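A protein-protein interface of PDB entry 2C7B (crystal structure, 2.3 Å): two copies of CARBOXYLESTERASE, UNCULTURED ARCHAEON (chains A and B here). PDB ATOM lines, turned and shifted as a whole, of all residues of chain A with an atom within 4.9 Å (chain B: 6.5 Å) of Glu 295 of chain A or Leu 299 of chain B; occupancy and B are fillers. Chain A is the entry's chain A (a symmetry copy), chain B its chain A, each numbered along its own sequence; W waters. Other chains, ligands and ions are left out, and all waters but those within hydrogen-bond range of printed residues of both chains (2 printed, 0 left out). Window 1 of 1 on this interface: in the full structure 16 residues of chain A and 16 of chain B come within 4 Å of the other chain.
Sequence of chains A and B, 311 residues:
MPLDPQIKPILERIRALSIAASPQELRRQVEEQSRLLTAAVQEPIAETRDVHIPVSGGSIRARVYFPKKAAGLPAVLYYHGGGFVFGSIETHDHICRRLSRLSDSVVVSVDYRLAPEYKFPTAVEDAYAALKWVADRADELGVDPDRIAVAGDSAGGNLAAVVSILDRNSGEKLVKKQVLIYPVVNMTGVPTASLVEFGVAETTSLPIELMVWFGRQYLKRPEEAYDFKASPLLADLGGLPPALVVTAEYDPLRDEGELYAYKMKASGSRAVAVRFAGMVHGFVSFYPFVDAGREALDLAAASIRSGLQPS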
ATOM      1  N   PHE A 276       9.339  10.719 -22.744  1.00  0.00           N
ATOM      2  CA  PHE A 276      10.624  11.071 -22.175  1.00  0.00           C
ATOM      3  C   PHE A 276      11.508   9.852 -22.062  1.00  0.00           C
ATOM      4  O   PHE A 276      11.147   8.856 -21.433  1.00  0.00           O
ATOM      5  CB  PHE A 276      10.436  11.721 -20.817  1.00  0.00           C
ATOM      6  CG  PHE A 276      10.092  13.172 -20.908  1.00  0.00           C
ATOM      7  CD1 PHE A 276       8.899  13.594 -21.482  1.00  0.00           C
ATOM      8  CD2 PHE A 276      11.015  14.123 -20.508  1.00  0.00           C
ATOM      9  CE1 PHE A 276       8.647  14.956 -21.663  1.00  0.00           C
ATOM     10  CE2 PHE A 276      10.783  15.478 -20.682  1.00  0.00           C
ATOM     11  CZ  PHE A 276       9.597  15.904 -21.261  1.00  0.00           C
ATOM     12  N   ASP A 291      16.773  15.923 -14.055  1.00  0.00           N
ATOM     13  CA  ASP A 291      16.671  16.973 -15.072  1.00  0.00           C
ATOM     14  C   ASP A 291      15.434  16.789 -15.947  1.00  0.00           C
ATOM     15  O   ASP A 291      14.692  17.729 -16.205  1.00  0.00           O
ATOM     16  CB  ASP A 291      17.924  17.018 -15.966  1.00  0.00           C
ATOM     17  CG  ASP A 291      19.233  16.941 -15.173  1.00  0.00           C
ATOM     18  OD1 ASP A 291      19.329  17.553 -14.085  1.00  0.00           O
ATOM     19  OD2 ASP A 291      20.175  16.259 -15.649  1.00  0.00           O
ATOM     20  N   ALA A 292      15.194  15.570 -16.389  1.00  0.00           N
ATOM     21  CA  ALA A 292      14.037  15.295 -17.232  1.00  0.00           C
ATOM     22  C   ALA A 292      12.688  15.652 -16.557  1.00  0.00           C
ATOM     23  O   ALA A 292      11.749  16.067 -17.238  1.00  0.00           O
ATOM     24  CB  ALA A 292      14.059  13.821 -17.662  1.00  0.00           C
ATOM     25  N   GLY A 293      12.585  15.512 -15.234  1.00  0.00           N
ATOM     26  CA  GLY A 293      11.336  15.847 -14.566  1.00  0.00           C
ATOM     27  C   GLY A 293      11.122  17.338 -14.716  1.00  0.00           C
ATOM     28  O   GLY A 293      10.008  17.826 -14.922  1.00  0.00           O
ATOM     29  N   ARG A 294      12.228  18.063 -14.644  1.00  0.00           N
ATOM     30  CA  ARG A 294      12.207  19.505 -14.769  1.00  0.00           C
ATOM     31  C   ARG A 294      11.877  19.947 -16.208  1.00  0.00           C
ATOM     32  O   ARG A 294      11.102  20.886 -16.400  1.00  0.00           O
ATOM     33  CB  ARG A 294      13.552  20.065 -14.316  1.00  0.00           C
ATOM     34  CG  ARG A 294      13.496  21.517 -13.877  1.00  0.00           C
ATOM     35  CD  ARG A 294      14.219  22.384 -14.885  1.00  0.00           C
ATOM     36  NE  ARG A 294      15.655  22.636 -14.663  1.00  0.00           N
ATOM     37  CZ  ARG A 294      16.500  21.975 -13.854  1.00  0.00           C
ATOM     38  NH1 ARG A 294      16.121  20.941 -13.090  1.00  0.00           N
ATOM     39  NH2 ARG A 294      17.774  22.367 -13.822  1.00  0.00           N
ATOM     40  N   GLU A 295      12.448  19.280 -17.216  1.00  0.00           N
ATOM     41  CA  GLU A 295      12.133  19.633 -18.599  1.00  0.00           C
ATOM     42  C   GLU A 295      10.654  19.320 -18.853  1.00  0.00           C
ATOM     43  O   GLU A 295       9.955  20.080 -19.520  1.00  0.00           O
ATOM     44  CB  GLU A 295      12.990  18.836 -19.586  1.00  0.00           C
ATOM     45  CG  GLU A 295      14.488  19.079 -19.492  1.00  0.00           C
ATOM     46  CD  GLU A 295      14.917  20.427 -20.053  1.00  0.00           C
ATOM     47  OE1 GLU A 295      14.070  21.178 -20.610  1.00  0.00           O
ATOM     48  OE2 GLU A 295      16.123  20.733 -19.929  1.00  0.00           O
ATOM     49  N   ALA A 296      10.172  18.203 -18.310  1.00  0.00           N
ATOM     50  CA  ALA A 296       8.771  17.824 -18.496  1.00  0.00           C
ATOM     51  C   ALA A 296       7.826  18.876 -17.912  1.00  0.00           C
ATOM     52  O   ALA A 296       6.817  19.242 -18.520  1.00  0.00           O
ATOM     53  CB  ALA A 296       8.502  16.476 -17.844  1.00  0.00           C
ATOM     54  N   LEU A 297       8.169  19.357 -16.727  1.00  0.00           N
ATOM     55  CA  LEU A 297       7.370  20.356 -16.033  1.00  0.00           C
ATOM     56  C   LEU A 297       7.315  21.671 -16.813  1.00  0.00           C
ATOM     57  O   LEU A 297       6.284  22.347 -16.856  1.00  0.00           O
ATOM     58  CB  LEU A 297       7.972  20.586 -14.651  1.00  0.00           C
ATOM     59  CG  LEU A 297       7.100  20.667 -13.403  1.00  0.00           C
ATOM     60  CD1 LEU A 297       5.792  19.944 -13.627  1.00  0.00           C
ATOM     61  CD2 LEU A 297       7.894  20.080 -12.220  1.00  0.00           C
ATOM     62  N   ASP A 298       8.434  22.031 -17.424  1.00  0.00           N
ATOM     63  CA  ASP A 298       8.505  23.258 -18.201  1.00  0.00           C
ATOM     64  C   ASP A 298       7.690  23.137 -19.500  1.00  0.00           C
ATOM     65  O   ASP A 298       7.127  24.116 -19.980  1.00  0.00           O
ATOM     66  CB  ASP A 298       9.981  23.608 -18.483  1.00  0.00           C
ATOM     67  CG  ASP A 298      10.703  24.200 -17.244  1.00  0.00           C
ATOM     68  OD1 ASP A 298      10.429  23.764 -16.090  1.00  0.00           O
ATOM     69  OD2 ASP A 298      11.560  25.101 -17.428  1.00  0.00           O
ATOM     70  N   LEU A 299       7.618  21.938 -20.064  1.00  0.00           N
ATOM     71  CA  LEU A 299       6.834  21.755 -21.276  1.00  0.00           C
ATOM     72  C   LEU A 299       5.364  21.941 -20.869  1.00  0.00           C
ATOM     73  O   LEU A 299       4.620  22.699 -21.503  1.00  0.00           O
ATOM     74  CB  LEU A 299       7.058  20.358 -21.848  1.00  0.00           C
ATOM     75  CG  LEU A 299       5.887  19.819 -22.667  1.00  0.00           C
ATOM     76  CD1 LEU A 299       5.725  20.583 -23.972  1.00  0.00           C
ATOM     77  CD2 LEU A 299       6.125  18.358 -22.928  1.00  0.00           C
ATOM     78  N   LYS B 177      24.170  25.842 -22.669  1.00  0.00           N
ATOM     79  CA  LYS B 177      23.128  24.857 -22.942  1.00  0.00           C
ATOM     80  C   LYS B 177      22.998  24.626 -24.454  1.00  0.00           C
ATOM     81  O   LYS B 177      23.330  25.507 -25.240  1.00  0.00           O
ATOM     82  CB  LYS B 177      21.789  25.336 -22.368  1.00  0.00           C
ATOM     83  CG  LYS B 177      20.682  24.333 -22.621  1.00  0.00           C
ATOM     84  CD  LYS B 177      19.554  24.399 -21.618  1.00  0.00           C
ATOM     85  CE  LYS B 177      18.874  23.033 -21.510  1.00  0.00           C
ATOM     86  NZ  LYS B 177      17.699  23.052 -20.590  1.00  0.00           N
ATOM     87  N   ALA B 243      22.292  19.174 -22.466  1.00  0.00           N
ATOM     88  CA  ALA B 243      21.609  19.009 -23.746  1.00  0.00           C
ATOM     89  C   ALA B 243      20.123  18.616 -23.652  1.00  0.00           C
ATOM     90  O   ALA B 243      19.718  17.825 -22.791  1.00  0.00           O
ATOM     91  CB  ALA B 243      22.322  18.001 -24.591  1.00  0.00           C
ATOM     92  N   LEU B 244      19.316  19.209 -24.539  1.00  0.00           N
ATOM     93  CA  LEU B 244      17.890  18.884 -24.657  1.00  0.00           C
ATOM     94  C   LEU B 244      17.832  18.339 -26.091  1.00  0.00           C
ATOM     95  O   LEU B 244      18.132  19.070 -27.044  1.00  0.00           O
ATOM     96  CB  LEU B 244      16.983  20.131 -24.551  1.00  0.00           C
ATOM     97  CG  LEU B 244      15.497  19.913 -24.181  1.00  0.00           C
ATOM     98  CD1 LEU B 244      14.609  20.398 -25.294  1.00  0.00           C
ATOM     99  CD2 LEU B 244      15.196  18.458 -23.891  1.00  0.00           C
ATOM    100  N   VAL B 245      17.497  17.059 -26.255  1.00  0.00           N
ATOM    101  CA  VAL B 245      17.431  16.488 -27.599  1.00  0.00           C
ATOM    102  C   VAL B 245      15.994  16.153 -27.959  1.00  0.00           C
ATOM    103  O   VAL B 245      15.296  15.433 -27.244  1.00  0.00           O
ATOM    104  CB  VAL B 245      18.308  15.195 -27.749  1.00  0.00           C
ATOM    105  CG1 VAL B 245      18.152  14.637 -29.157  1.00  0.00           C
ATOM    106  CG2 VAL B 245      19.782  15.508 -27.494  1.00  0.00           C
ATOM    107  N   VAL B 246      15.551  16.694 -29.083  1.00  0.00           N
ATOM    108  CA  VAL B 246      14.193  16.462 -29.544  1.00  0.00           C
ATOM    109  C   VAL B 246      14.161  15.599 -30.806  1.00  0.00           C
ATOM    110  O   VAL B 246      14.807  15.918 -31.801  1.00  0.00           O
ATOM    111  CB  VAL B 246      13.481  17.810 -29.814  1.00  0.00           C
ATOM    112  CG1 VAL B 246      12.124  17.565 -30.490  1.00  0.00           C
ATOM    113  CG2 VAL B 246      13.289  18.568 -28.480  1.00  0.00           C
ATOM    114  N   VAL B 272      18.732  15.297 -22.008  1.00  0.00           N
ATOM    115  CA  VAL B 272      17.368  14.825 -21.886  1.00  0.00           C
ATOM    116  C   VAL B 272      16.850  14.684 -23.291  1.00  0.00           C
ATOM    117  O   VAL B 272      17.001  15.604 -24.095  1.00  0.00           O
ATOM    118  CB  VAL B 272      16.500  15.821 -21.125  1.00  0.00           C
ATOM    119  CG1 VAL B 272      15.027  15.439 -21.277  1.00  0.00           C
ATOM    120  CG2 VAL B 272      16.917  15.852 -19.656  1.00  0.00           C
ATOM    121  N   VAL B 274      13.542  13.817 -25.853  1.00  0.00           N
ATOM    122  CA  VAL B 274      12.087  13.788 -25.893  1.00  0.00           C
ATOM    123  C   VAL B 274      11.621  13.296 -27.257  1.00  0.00           C
ATOM    124  O   VAL B 274      12.062  13.810 -28.286  1.00  0.00           O
ATOM    125  CB  VAL B 274      11.529  15.177 -25.661  1.00  0.00           C
ATOM    126  CG1 VAL B 274      10.050  15.094 -25.474  1.00  0.00           C
ATOM    127  CG2 VAL B 274      12.203  15.791 -24.442  1.00  0.00           C
ATOM    128  N   PHE B 276       8.622  12.939 -29.920  1.00  0.00           N
ATOM    129  CA  PHE B 276       7.278  13.372 -30.241  1.00  0.00           C
ATOM    130  C   PHE B 276       6.566  12.330 -31.070  1.00  0.00           C
ATOM    131  O   PHE B 276       7.033  11.936 -32.140  1.00  0.00           O
ATOM    132  CB  PHE B 276       7.314  14.701 -30.971  1.00  0.00           C
ATOM    133  CG  PHE B 276       7.459  15.869 -30.050  1.00  0.00           C
ATOM    134  CD1 PHE B 276       8.606  16.046 -29.287  1.00  0.00           C
ATOM    135  CD2 PHE B 276       6.396  16.739 -29.872  1.00  0.00           C
ATOM    136  CE1 PHE B 276       8.675  17.077 -28.346  1.00  0.00           C
ATOM    137  CE2 PHE B 276       6.447  17.766 -28.943  1.00  0.00           C
ATOM    138  CZ  PHE B 276       7.586  17.942 -28.173  1.00  0.00           C
ATOM    139  N   ARG B 294       4.396  23.115 -32.466  1.00  0.00           N
ATOM    140  CA  ARG B 294       4.223  24.211 -31.537  1.00  0.00           C
ATOM    141  C   ARG B 294       4.551  23.789 -30.092  1.00  0.00           C
ATOM    142  O   ARG B 294       5.197  24.545 -29.362  1.00  0.00           O
ATOM    143  CB  ARG B 294       2.795  24.738 -31.645  1.00  0.00           C
ATOM    144  CG  ARG B 294       2.631  26.169 -31.170  1.00  0.00           C
ATOM    145  CD  ARG B 294       1.839  26.193 -29.880  1.00  0.00           C
ATOM    146  NE  ARG B 294       0.374  26.325 -29.981  1.00  0.00           N
ATOM    147  CZ  ARG B 294      -0.406  26.138 -31.058  1.00  0.00           C
ATOM    148  NH1 ARG B 294       0.079  25.793 -32.259  1.00  0.00           N
ATOM    149  NH2 ARG B 294      -1.722  26.297 -30.914  1.00  0.00           N
ATOM    150  N   GLU B 295       4.123  22.594 -29.674  1.00  0.00           N
ATOM    151  CA  GLU B 295       4.446  22.130 -28.326  1.00  0.00           C
ATOM    152  C   GLU B 295       5.964  21.935 -28.233  1.00  0.00           C
ATOM    153  O   GLU B 295       6.580  22.264 -27.220  1.00  0.00           O
ATOM    154  CB  GLU B 295       3.752  20.802 -28.012  1.00  0.00           C
ATOM    155  CG  GLU B 295       2.231  20.845 -28.016  1.00  0.00           C
ATOM    156  CD  GLU B 295       1.646  21.554 -26.802  1.00  0.00           C
ATOM    157  OE1 GLU B 295       2.404  21.958 -25.879  1.00  0.00           O
ATOM    158  OE2 GLU B 295       0.404  21.705 -26.782  1.00  0.00           O
ATOM    159  N   ALA B 296       6.571  21.410 -29.296  1.00  0.00           N
ATOM    160  CA  ALA B 296       8.018  21.192 -29.300  1.00  0.00           C
ATOM    161  C   ALA B 296       8.782  22.506 -29.133  1.00  0.00           C
ATOM    162  O   ALA B 296       9.757  22.592 -28.382  1.00  0.00           O
ATOM    163  CB  ALA B 296       8.441  20.513 -30.595  1.00  0.00           C
ATOM    164  N   LEU B 297       8.325  23.527 -29.843  1.00  0.00           N
ATOM    165  CA  LEU B 297       8.947  24.842 -29.803  1.00  0.00           C
ATOM    166  C   LEU B 297       8.854  25.465 -28.408  1.00  0.00           C
ATOM    167  O   LEU B 297       9.783  26.128 -27.941  1.00  0.00           O
ATOM    168  CB  LEU B 297       8.259  25.736 -30.829  1.00  0.00           C
ATOM    169  CG  LEU B 297       9.056  26.637 -31.765  1.00  0.00           C
ATOM    170  CD1 LEU B 297      10.459  26.105 -31.938  1.00  0.00           C
ATOM    171  CD2 LEU B 297       8.300  26.732 -33.104  1.00  0.00           C
ATOM    172  N   ASP B 298       7.723  25.251 -27.751  1.00  0.00           N
ATOM    173  CA  ASP B 298       7.518  25.787 -26.415  1.00  0.00           C
ATOM    174  C   ASP B 298       8.398  25.057 -25.387  1.00  0.00           C
ATOM    175  O   ASP B 298       8.841  25.651 -24.408  1.00  0.00           O
ATOM    176  CB  ASP B 298       6.022  25.704 -26.048  1.00  0.00           C
ATOM    177  CG  ASP B 298       5.171  26.793 -26.754  1.00  0.00           C
ATOM    178  OD1 ASP B 298       5.452  27.140 -27.938  1.00  0.00           O
ATOM    179  OD2 ASP B 298       4.207  27.296 -26.125  1.00  0.00           O
ATOM    180  N   LEU B 299       8.659  23.775 -25.608  1.00  0.00           N
ATOM    181  CA  LEU B 299       9.514  23.041 -24.687  1.00  0.00           C
ATOM    182  C   LEU B 299      10.925  23.627 -24.849  1.00  0.00           C
ATOM    183  O   LEU B 299      11.584  23.979 -23.863  1.00  0.00           O
ATOM    184  CB  LEU B 299       9.510  21.553 -25.030  1.00  0.00           C
ATOM    185  CG  LEU B 299      10.779  20.811 -24.617  1.00  0.00           C
ATOM    186  CD1 LEU B 299      10.891  20.703 -23.104  1.00  0.00           C
ATOM    187  CD2 LEU B 299      10.756  19.448 -25.251  1.00  0.00           C
ATOM    188  N   ALA B 300      11.368  23.743 -26.101  1.00  0.00           N
ATOM    189  CA  ALA B 300      12.687  24.292 -26.415  1.00  0.00           C
ATOM    190  C   ALA B 300      12.861  25.678 -25.797  1.00  0.00           C
ATOM    191  O   ALA B 300      13.861  25.934 -25.134  1.00  0.00           O
ATOM    192  CB  ALA B 300      12.882  24.372 -27.930  1.00  0.00           C
ATOM    193  N   ALA B 301      11.907  26.577 -26.015  1.00  0.00           N
ATOM    194  CA  ALA B 301      12.032  27.919 -25.445  1.00  0.00           C
ATOM    195  C   ALA B 301      12.051  27.870 -23.907  1.00  0.00           C
ATOM    196  O   ALA B 301      12.759  28.643 -23.260  1.00  0.00           O
ATOM    197  CB  ALA B 301      10.885  28.848 -25.944  1.00  0.00           C
ATOM    198  N   ALA B 302      11.291  26.954 -23.322  1.00  0.00           N
ATOM    199  CA  ALA B 302      11.266  26.865 -21.874  1.00  0.00           C
ATOM    200  C   ALA B 302      12.568  26.247 -21.361  1.00  0.00           C
ATOM    201  O   ALA B 302      13.063  26.612 -20.296  1.00  0.00           O
ATOM    202  CB  ALA B 302      10.071  26.040 -21.422  1.00  0.00           C
ATOM    203  N   SER B 303      13.120  25.320 -22.136  1.00  0.00           N
ATOM    204  CA  SER B 303      14.357  24.646 -21.776  1.00  0.00           C
ATOM    205  C   SER B 303      15.509  25.660 -21.826  1.00  0.00           C
ATOM    206  O   SER B 303      16.384  25.675 -20.963  1.00  0.00           O
ATOM    207  CB  SER B 303      14.596  23.480 -22.749  1.00  0.00           C
ATOM    208  OG  SER B 303      15.653  22.637 -22.318  1.00  0.00           O
ATOM    209  N   ILE B 304      15.509  26.515 -22.835  1.00  0.00           N
ATOM    210  CA  ILE B 304      16.551  27.529 -22.911  1.00  0.00           C
ATOM    211  C   ILE B 304      16.409  28.514 -21.746  1.00  0.00           C
ATOM    212  O   ILE B 304      17.382  28.796 -21.043  1.00  0.00           O
ATOM    213  CB  ILE B 304      16.452  28.324 -24.207  1.00  0.00           C
ATOM    214  CG1 ILE B 304      17.169  27.560 -25.304  1.00  0.00           C
ATOM    215  CG2 ILE B 304      16.925  29.764 -23.989  1.00  0.00           C
ATOM    216  CD1 ILE B 304      16.440  27.679 -26.604  1.00  0.00           C
ATOM    217  N   SER B 306      15.124  28.313 -18.782  1.00  0.00           N
ATOM    218  CA  SER B 306      15.617  27.737 -17.543  1.00  0.00           C
ATOM    219  C   SER B 306      17.124  27.454 -17.573  1.00  0.00           C
ATOM    220  O   SER B 306      17.806  27.632 -16.562  1.00  0.00           O
ATOM    221  CB  SER B 306      14.859  26.436 -17.224  1.00  0.00           C
ATOM    222  OG  SER B 306      15.481  25.286 -17.802  1.00  0.00           O
HETATM  223  O   HOH W   1      13.300  23.571 -18.532  1.00  0.00           O
HETATM  224  O   HOH W   2      11.073  27.961 -18.430  1.00  0.00           O
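Among the printed residues, pairs that only touch across the chains: Asp 291 of chain A with Val 272 of chain B, Ala 292 of chain A with Val 272 of chain B, Glu 295 of chain A with Leu 299 of chain B, Asp 298 of chain A with Ala 302 of chain B, Asp 298 of chain A with Ser 306 of chain B and Leu 299 of chain A with Glu 295 of chain B.
Water W1 lies within hydrogen-bond range of the side-chain carboxylate (OD2) of Asp 298 of chain A (2.6 Å), the side-chain hydroxyl (OG) of Ser 306 of chain B (2.9 Å) and the side-chain carboxylate (OE1) of Glu 295 of chain A (3.3 Å).
Water W2 lies within hydrogen-bond range of the backbone carbonyl oxygen (O) of Ala 302 of chain B and the side-chain carboxylate (OD2) of Asp 298 of chain A.
Of chain B, only Lys 177, Leu 299 and Ser 303 come within 4 Å of Glu 295 of chain A.
Of the printed residues of chain B, Leu 299 of chain A touches Glu 295 (3.8 Å).
Of the printed residues of chain A, Val 272 of chain B touches Asp 291 and Ala 292.
Leu 299 of chain B touches just one residue of chain A: Glu 295 (3.8 Å).
Printed residues of chain A within 4 Å of Ser 306 of chain B: Asp 298 (3.6 Å).
The side-chain carboxylate of Glu 295 of chain A lies within salt-bridge range of the side-chain amino group of Lys 177 of chain B (2.9 Å).
OG of Ser 303 of chain B is in hydrogen-bond range of OE1 of Glu 295 of chain A (2.7 Å).
The side-chain amino group of Lys 177 of chain B lies within hydrogen-bond range of the side-chain hydroxyl of Ser 303 of chain B, 2.7 Å away.
The backbone carbonyl oxygen of Ala 243 of chain B lies within hydrogen-bond range of the backbone NH of Val 272 of chain B, 2.8 Å away.
The backbone carbonyl oxygen (O) of Val 272 of chain B is in hydrogen-bond range of the backbone NH (N) of Val 245 of chain B (2.7 Å).
O of Ser 303 of chain B lies within hydrogen-bond range of OG of Ser 306 of chain B (3.3 Å).
Glu 295 of chain A touches Leu 299 of chain B, and with the chains exchanged Leu 299 of chain A touches Glu 295 of chain B.
7 positions are printed for both chains.
Of the 8 pairs that touch across the chains among the printed residues, 2 have their exchanged pair printed and touching as well.
Of the 20 printed residues of chain B, 7 touch a printed residue of chain A.
Printed residues of chain B that touch a printed residue of chain A: Lys 177, Val 272, Glu 295, Leu 299, Ala 302, Ser 303 and Ser 306.
Hydrophobic or aromatic side chains of chain B within 4 Å of the printed part of chain A: Val 272, Leu 299 and Ala 302.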
